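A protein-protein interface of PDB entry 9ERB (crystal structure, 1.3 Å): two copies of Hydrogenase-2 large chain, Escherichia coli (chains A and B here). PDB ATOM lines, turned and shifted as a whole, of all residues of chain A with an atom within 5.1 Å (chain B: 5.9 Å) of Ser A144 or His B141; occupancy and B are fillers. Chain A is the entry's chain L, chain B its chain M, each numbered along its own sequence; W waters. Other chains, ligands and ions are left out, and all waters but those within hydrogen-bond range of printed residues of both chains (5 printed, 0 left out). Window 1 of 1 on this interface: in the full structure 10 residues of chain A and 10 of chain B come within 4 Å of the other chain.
The side-chain hydroxyl (OG) of Ser B144 sits at hydrogen-bond distance from the backbone carbonyl oxygen (O) of His A141, 3.3 Å away.
The side-chain hydroxyl (OG) of Ser A144 is in hydrogen-bond range of the backbone carbonyl oxygen (O) of His B141 (3.4 Å).
The side-chain carboxylate (OE2) of Glu A146 is in salt-bridge range of the side-chain amino group (NZ) of Lys B135 (2.9 Å).
OE1 of Glu A147 lies within hydrogen-bond range of ND1 of His B141 (2.7 Å).
N of Glu A146 sits close to OG of Ser A144.
OG of Ser A144 lies within hydrogen-bond range of N of Glu A147 (2.9 Å).
The side-chain hydroxyl (OG1) of Thr A149 lies within hydrogen-bond range of the backbone carbonyl oxygen (O) of Pro A145, at 2.8 Å.
The side-chain carboxylate (OE1) of Glu A147 is in salt-bridge range of the side-chain amino group (NZ) of Lys A150 (2.7 Å).
Among the printed residues, pairs that only touch across the chains: Glu A146 with Thr B139, Glu A146 with Trp B140, His A141 with Leu B142, Leu A142 with Leu B142, Leu A142 with His B141, Lys A150 with His B141 and Pro A145 with Lys B135.
Of the printed residues of chain B, His A141 touches Leu B142 and Ser B144.
Asn A143 touches none of the printed residues of chain B.
Ser A144 touches one residue of chain B.
Of the printed residues of chain B, Glu A146 touches Lys B135, Thr B139 and Trp B140.
Printed residues of chain A within 4 Å of Trp B140: Glu A146.
Of the printed residues of chain A, His B141 touches Leu A142, Ser A144, Glu A147 and Lys A150.
Of the printed residues of chain A, Leu B142 touches His A141 and Leu A142.
The nearest residue of chain B that does not touch Ser A144 is Ser B144 (4.02 Å).
The nearest printed residue of chain B that does not touch Glu A147 is Trp B140 (5.4 Å).
Hydrophobic or aromatic side chains of chain B within 4 Å of the printed part of chain A: His B141 and Leu B142.
Hydrophobic or aromatic side chains of chain A that line the printed part of chain B: His A141, Leu A142 and Pro A145.
Among the printed residues, 11 pairs touch across the chains.
His A141 touches Leu B142, and with the chains exchanged Leu A142 touches His B141.
His A141 touches Ser B144, and with the chains exchanged Ser A144 touches His B141.
Leu A142 touches its own counterpart, Leu B142.
Of the 11 pairs that touch across the chains among the printed residues, 5 have their exchanged pair printed and touching as well.
Water W5 bridges the side-chain carboxylate of Glu A146 (2.7 Å) and the backbone carbonyl oxygen of Asn B143 (3.3 Å).
Water W2 lies within hydrogen-bond range of O of His A141 (2.7 Å), O of His B141 (2.8 Å), OG of Ser A144 (3.0 Å) and N of Asn A143 (3.4 Å).
Water W1 lies within hydrogen-bond range of OE2 of Glu A147 (2.7 Å) and ND1 of His B141 (3.3 Å).
Water W4 lies within hydrogen-bond range of O of Trp B140 (2.7 Å), OG of Ser A144 (2.9 Å), N of Asn B143 (2.9 Å), O of His B141 (3.2 Å) and N of Leu B142 (3.4 Å).
Water W3 lies within hydrogen-bond range of N of Asn A143 (2.9 Å), OG of Ser B144 (2.9 Å), O of His A141 (3.2 Å) and N of Leu A142 (3.4 Å).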
ATOM      1  N   SER A 131      -7.670  -3.282  26.463  1.00  0.00           N
ATOM      2  CA  SER A 131      -7.616  -4.103  25.264  1.00  0.00           C
ATOM      3  C   SER A 131      -8.688  -3.683  24.263  1.00  0.00           C
ATOM      4  O   SER A 131      -8.450  -3.653  23.048  1.00  0.00           O
ATOM      5  CB  SER A 131      -7.809  -5.575  25.663  1.00  0.00           C
ATOM      6  OG  SER A 131      -7.742  -6.420  24.550  1.00  0.00           O
ATOM      7  N   HIS A 141      -0.904  -9.301  18.284  1.00  0.00           N
ATOM      8  CA  HIS A 141      -1.374 -10.496  18.977  1.00  0.00           C
ATOM      9  C   HIS A 141      -1.165 -10.476  20.496  1.00  0.00           C
ATOM     10  O   HIS A 141      -1.601 -11.431  21.166  1.00  0.00           O
ATOM     11  CB  HIS A 141      -0.774 -11.759  18.341  1.00  0.00           C
ATOM     12  CG  HIS A 141       0.687 -11.983  18.628  1.00  0.00           C
ATOM     13  ND1 HIS A 141       1.231 -13.246  18.642  1.00  0.00           N
ATOM     14  CD2 HIS A 141       1.709 -11.138  18.894  1.00  0.00           C
ATOM     15  CE1 HIS A 141       2.528 -13.180  18.899  1.00  0.00           C
ATOM     16  NE2 HIS A 141       2.841 -11.904  19.050  1.00  0.00           N
ATOM     17  N   LEU A 142      -0.556  -9.432  21.069  1.00  0.00           N
ATOM     18  CA  LEU A 142      -0.222  -9.359  22.481  1.00  0.00           C
ATOM     19  C   LEU A 142      -0.847  -8.141  23.159  1.00  0.00           C
ATOM     20  O   LEU A 142      -0.241  -7.459  23.997  1.00  0.00           O
ATOM     21  CB  LEU A 142       1.289  -9.435  22.670  1.00  0.00           C
ATOM     22  CG  LEU A 142       1.840 -10.865  22.666  1.00  0.00           C
ATOM     23  CD1 LEU A 142       3.359 -10.880  22.601  1.00  0.00           C
ATOM     24  CD2 LEU A 142       1.404 -11.652  23.890  1.00  0.00           C
ATOM     25  N   ASN A 143      -2.119  -7.892  22.830  1.00  0.00           N
ATOM     26  CA  ASN A 143      -2.892  -6.810  23.418  1.00  0.00           C
ATOM     27  C   ASN A 143      -4.072  -7.326  24.229  1.00  0.00           C
ATOM     28  O   ASN A 143      -5.014  -6.567  24.471  1.00  0.00           O
ATOM     29  CB  ASN A 143      -3.388  -5.853  22.327  1.00  0.00           C
ATOM     30  CG  ASN A 143      -2.330  -4.873  21.879  1.00  0.00           C
ATOM     31  OD1 ASN A 143      -1.424  -4.526  22.650  1.00  0.00           O
ATOM     32  ND2 ASN A 143      -2.439  -4.431  20.628  1.00  0.00           N
ATOM     33  N   SER A 144      -4.039  -8.580  24.683  1.00  0.00           N
ATOM     34  CA  SER A 144      -5.186  -9.138  25.377  1.00  0.00           C
ATOM     35  C   SER A 144      -5.300  -8.564  26.785  1.00  0.00           C
ATOM     36  O   SER A 144      -4.312  -8.121  27.376  1.00  0.00           O
ATOM     37  CB  SER A 144      -5.094 -10.667  25.496  1.00  0.00           C
ATOM     38  OG  SER A 144      -4.005 -11.023  26.343  1.00  0.00           O
ATOM     39  N   PRO A 145      -6.500  -8.653  27.397  1.00  0.00           N
ATOM     40  CA  PRO A 145      -6.602  -8.306  28.816  1.00  0.00           C
ATOM     41  C   PRO A 145      -5.660  -9.107  29.668  1.00  0.00           C
ATOM     42  O   PRO A 145      -5.159  -8.608  30.669  1.00  0.00           O
ATOM     43  CB  PRO A 145      -8.073  -8.590  29.147  1.00  0.00           C
ATOM     44  CG  PRO A 145      -8.777  -8.420  27.831  1.00  0.00           C
ATOM     45  CD  PRO A 145      -7.810  -9.007  26.816  1.00  0.00           C
ATOM     46  N   GLU A 146      -5.428 -10.368  29.304  1.00  0.00           N
ATOM     47  CA  GLU A 146      -4.578 -11.222  30.116  1.00  0.00           C
ATOM     48  C   GLU A 146      -3.119 -10.774  30.062  1.00  0.00           C
ATOM     49  O   GLU A 146      -2.455 -10.728  31.101  1.00  0.00           O
ATOM     50  CB  GLU A 146      -4.710 -12.684  29.652  1.00  0.00           C
ATOM     51  CG  GLU A 146      -6.078 -13.341  29.903  1.00  0.00           C
ATOM     52  CD  GLU A 146      -7.225 -12.852  29.049  1.00  0.00           C
ATOM     53  OE1 GLU A 146      -7.034 -12.207  27.986  1.00  0.00           O
ATOM     54  OE2 GLU A 146      -8.380 -13.183  29.416  1.00  0.00           O
ATOM     55  N   GLU A 147      -2.634 -10.377  28.867  1.00  0.00           N
ATOM     56  CA  GLU A 147      -1.304  -9.774  28.778  1.00  0.00           C
ATOM     57  C   GLU A 147      -1.230  -8.532  29.642  1.00  0.00           C
ATOM     58  O   GLU A 147      -0.276  -8.335  30.415  1.00  0.00           O
ATOM     59  CB  GLU A 147      -0.986  -9.445  27.333  1.00  0.00           C
ATOM     60  CG  GLU A 147       0.322  -8.694  27.110  1.00  0.00           C
ATOM     61  CD  GLU A 147       1.590  -9.518  27.327  1.00  0.00           C
ATOM     62  OE1 GLU A 147       1.510 -10.698  27.757  1.00  0.00           O
ATOM     63  OE2 GLU A 147       2.694  -8.999  27.019  1.00  0.00           O
ATOM     64  N   PHE A 148      -2.228  -7.662  29.510  1.00  0.00           N
ATOM     65  CA  PHE A 148      -2.167  -6.396  30.211  1.00  0.00           C
ATOM     66  C   PHE A 148      -2.281  -6.584  31.725  1.00  0.00           C
ATOM     67  O   PHE A 148      -1.672  -5.838  32.485  1.00  0.00           O
ATOM     68  CB  PHE A 148      -3.258  -5.450  29.721  1.00  0.00           C
ATOM     69  CG  PHE A 148      -3.097  -4.977  28.286  1.00  0.00           C
ATOM     70  CD1 PHE A 148      -1.892  -5.080  27.604  1.00  0.00           C
ATOM     71  CD2 PHE A 148      -4.157  -4.354  27.645  1.00  0.00           C
ATOM     72  CE1 PHE A 148      -1.769  -4.609  26.302  1.00  0.00           C
ATOM     73  CE2 PHE A 148      -4.020  -3.859  26.359  1.00  0.00           C
ATOM     74  CZ  PHE A 148      -2.815  -4.000  25.680  1.00  0.00           C
ATOM     75  N   THR A 149      -3.061  -7.581  32.188  1.00  0.00           N
ATOM     76  CA  THR A 149      -3.139  -7.867  33.620  1.00  0.00           C
ATOM     77  C   THR A 149      -1.805  -8.346  34.174  1.00  0.00           C
ATOM     78  O   THR A 149      -1.399  -7.953  35.265  1.00  0.00           O
ATOM     79  CB  THR A 149      -4.242  -8.907  33.869  1.00  0.00           C
ATOM     80  OG1 THR A 149      -5.502  -8.410  33.402  1.00  0.00           O
ATOM     81  CG2 THR A 149      -4.347  -9.260  35.365  1.00  0.00           C
ATOM     82  N   LYS A 150      -1.105  -9.200  33.431  1.00  0.00           N
ATOM     83  CA  LYS A 150       0.210  -9.662  33.882  1.00  0.00           C
ATOM     84  C   LYS A 150       1.177  -8.499  34.015  1.00  0.00           C
ATOM     85  O   LYS A 150       1.907  -8.372  35.009  1.00  0.00           O
ATOM     86  CB  LYS A 150       0.737 -10.675  32.877  1.00  0.00           C
ATOM     87  CG  LYS A 150       2.121 -11.188  33.170  1.00  0.00           C
ATOM     88  CD  LYS A 150       2.545 -12.290  32.180  1.00  0.00           C
ATOM     89  CE  LYS A 150       2.071 -12.061  30.723  1.00  0.00           C
ATOM     90  NZ  LYS A 150       3.061 -11.354  29.911  1.00  0.00           N
ATOM     91  N   LYS B 135     -12.372 -16.872  28.916  1.00  0.00           N
ATOM     92  CA  LYS B 135     -12.332 -15.974  30.068  1.00  0.00           C
ATOM     93  C   LYS B 135     -12.703 -16.728  31.337  1.00  0.00           C
ATOM     94  O   LYS B 135     -13.674 -17.486  31.349  1.00  0.00           O
ATOM     95  CB  LYS B 135     -13.362 -14.878  29.851  1.00  0.00           C
ATOM     96  CG  LYS B 135     -13.121 -14.042  28.661  1.00  0.00           C
ATOM     97  CD  LYS B 135     -11.833 -13.260  28.786  1.00  0.00           C
ATOM     98  CE  LYS B 135     -11.479 -12.618  27.467  1.00  0.00           C
ATOM     99  NZ  LYS B 135     -10.226 -11.837  27.631  1.00  0.00           N
ATOM    100  N   THR B 139      -5.577 -17.782  32.024  1.00  0.00           N
ATOM    101  CA  THR B 139      -4.933 -16.474  32.028  1.00  0.00           C
ATOM    102  C   THR B 139      -3.828 -16.368  30.976  1.00  0.00           C
ATOM    103  O   THR B 139      -3.062 -15.405  31.004  1.00  0.00           O
ATOM    104  CB  THR B 139      -4.338 -16.154  33.406  1.00  0.00           C
ATOM    105  OG1 THR B 139      -3.279 -17.077  33.706  1.00  0.00           O
ATOM    106  CG2 THR B 139      -5.392 -16.220  34.507  1.00  0.00           C
ATOM    107  N   TRP B 140      -3.718 -17.325  30.077  1.00  0.00           N
ATOM    108  CA  TRP B 140      -2.686 -17.299  29.051  1.00  0.00           C
ATOM    109  C   TRP B 140      -2.762 -16.020  28.252  1.00  0.00           C
ATOM    110  O   TRP B 140      -3.851 -15.558  27.890  1.00  0.00           O
ATOM    111  CB  TRP B 140      -2.921 -18.456  28.100  1.00  0.00           C
ATOM    112  CG  TRP B 140      -2.004 -18.624  26.928  1.00  0.00           C
ATOM    113  CD1 TRP B 140      -2.373 -18.802  25.628  1.00  0.00           C
ATOM    114  CD2 TRP B 140      -0.549 -18.764  26.943  1.00  0.00           C
ATOM    115  NE1 TRP B 140      -1.273 -19.037  24.838  1.00  0.00           N
ATOM    116  CE2 TRP B 140      -0.148 -19.036  25.619  1.00  0.00           C
ATOM    117  CE3 TRP B 140       0.435 -18.743  27.952  1.00  0.00           C
ATOM    118  CZ2 TRP B 140       1.185 -19.224  25.266  1.00  0.00           C
ATOM    119  CZ3 TRP B 140       1.764 -18.960  27.583  1.00  0.00           C
ATOM    120  CH2 TRP B 140       2.116 -19.194  26.271  1.00  0.00           C
ATOM    121  N   HIS B 141      -1.588 -15.488  27.917  1.00  0.00           N
ATOM    122  CA  HIS B 141      -1.519 -14.181  27.271  1.00  0.00           C
ATOM    123  C   HIS B 141      -1.648 -14.223  25.752  1.00  0.00           C
ATOM    124  O   HIS B 141      -1.624 -13.143  25.132  1.00  0.00           O
ATOM    125  CB  HIS B 141      -0.229 -13.474  27.667  1.00  0.00           C
ATOM    126  CG  HIS B 141       1.016 -14.042  27.074  1.00  0.00           C
ATOM    127  ND1 HIS B 141       2.132 -13.247  26.938  1.00  0.00           N
ATOM    128  CD2 HIS B 141       1.375 -15.272  26.627  1.00  0.00           C
ATOM    129  CE1 HIS B 141       3.108 -13.952  26.401  1.00  0.00           C
ATOM    130  NE2 HIS B 141       2.689 -15.193  26.222  1.00  0.00           N
ATOM    131  N   LEU B 142      -1.824 -15.384  25.134  1.00  0.00           N
ATOM    132  CA  LEU B 142      -1.890 -15.518  23.687  1.00  0.00           C
ATOM    133  C   LEU B 142      -3.187 -16.191  23.228  1.00  0.00           C
ATOM    134  O   LEU B 142      -3.196 -17.024  22.311  1.00  0.00           O
ATOM    135  CB  LEU B 142      -0.648 -16.211  23.141  1.00  0.00           C
ATOM    136  CG  LEU B 142       0.573 -15.301  22.968  1.00  0.00           C
ATOM    137  CD1 LEU B 142       1.833 -16.101  22.715  1.00  0.00           C
ATOM    138  CD2 LEU B 142       0.334 -14.291  21.840  1.00  0.00           C
ATOM    139  N   ASN B 143      -4.297 -15.774  23.860  1.00  0.00           N
ATOM    140  CA  ASN B 143      -5.634 -16.215  23.473  1.00  0.00           C
ATOM    141  C   ASN B 143      -6.493 -15.091  22.904  1.00  0.00           C
ATOM    142  O   ASN B 143      -7.725 -15.186  22.906  1.00  0.00           O
ATOM    143  CB  ASN B 143      -6.357 -16.845  24.657  1.00  0.00           C
ATOM    144  CG  ASN B 143      -5.901 -18.271  24.932  1.00  0.00           C
ATOM    145  OD1 ASN B 143      -5.520 -19.012  24.037  1.00  0.00           O
ATOM    146  ND2 ASN B 143      -5.959 -18.648  26.198  1.00  0.00           N
ATOM    147  N   SER B 144      -5.878 -14.014  22.409  1.00  0.00           N
ATOM    148  CA  SER B 144      -6.663 -12.898  21.895  1.00  0.00           C
ATOM    149  C   SER B 144      -7.343 -13.247  20.574  1.00  0.00           C
ATOM    150  O   SER B 144      -6.901 -14.124  19.827  1.00  0.00           O
ATOM    151  CB  SER B 144      -5.764 -11.686  21.663  1.00  0.00           C
ATOM    152  OG  SER B 144      -4.856 -11.968  20.638  1.00  0.00           O
ATOM    153  N   GLN B 256      -1.339 -22.886  31.696  1.00  0.00           N
ATOM    154  CA  GLN B 256      -2.382 -22.007  31.178  1.00  0.00           C
ATOM    155  C   GLN B 256      -2.929 -22.464  29.840  1.00  0.00           C
ATOM    156  O   GLN B 256      -3.972 -21.959  29.408  1.00  0.00           O
ATOM    157  CB  GLN B 256      -1.837 -20.572  31.026  1.00  0.00           C
ATOM    158  CG  GLN B 256      -1.341 -20.022  32.354  1.00  0.00           C
ATOM    159  CD  GLN B 256      -0.525 -18.746  32.254  1.00  0.00           C
ATOM    160  OE1 GLN B 256      -0.354 -18.173  31.177  1.00  0.00           O
ATOM    161  NE2 GLN B 256       0.027 -18.335  33.383  1.00  0.00           N
HETATM  162  O   HOH W   1       4.488 -11.030  26.556  1.00  0.00           O
HETATM  163  O   HOH W   2      -2.812 -11.122  23.580  1.00  0.00           O
HETATM  164  O   HOH W   3      -3.921  -9.202  20.981  1.00  0.00           O
HETATM  165  O   HOH W   4      -4.682 -13.803  25.943  1.00  0.00           O
HETATM  166  O   HOH W   5      -7.474 -13.399  25.635  1.00  0.00           O
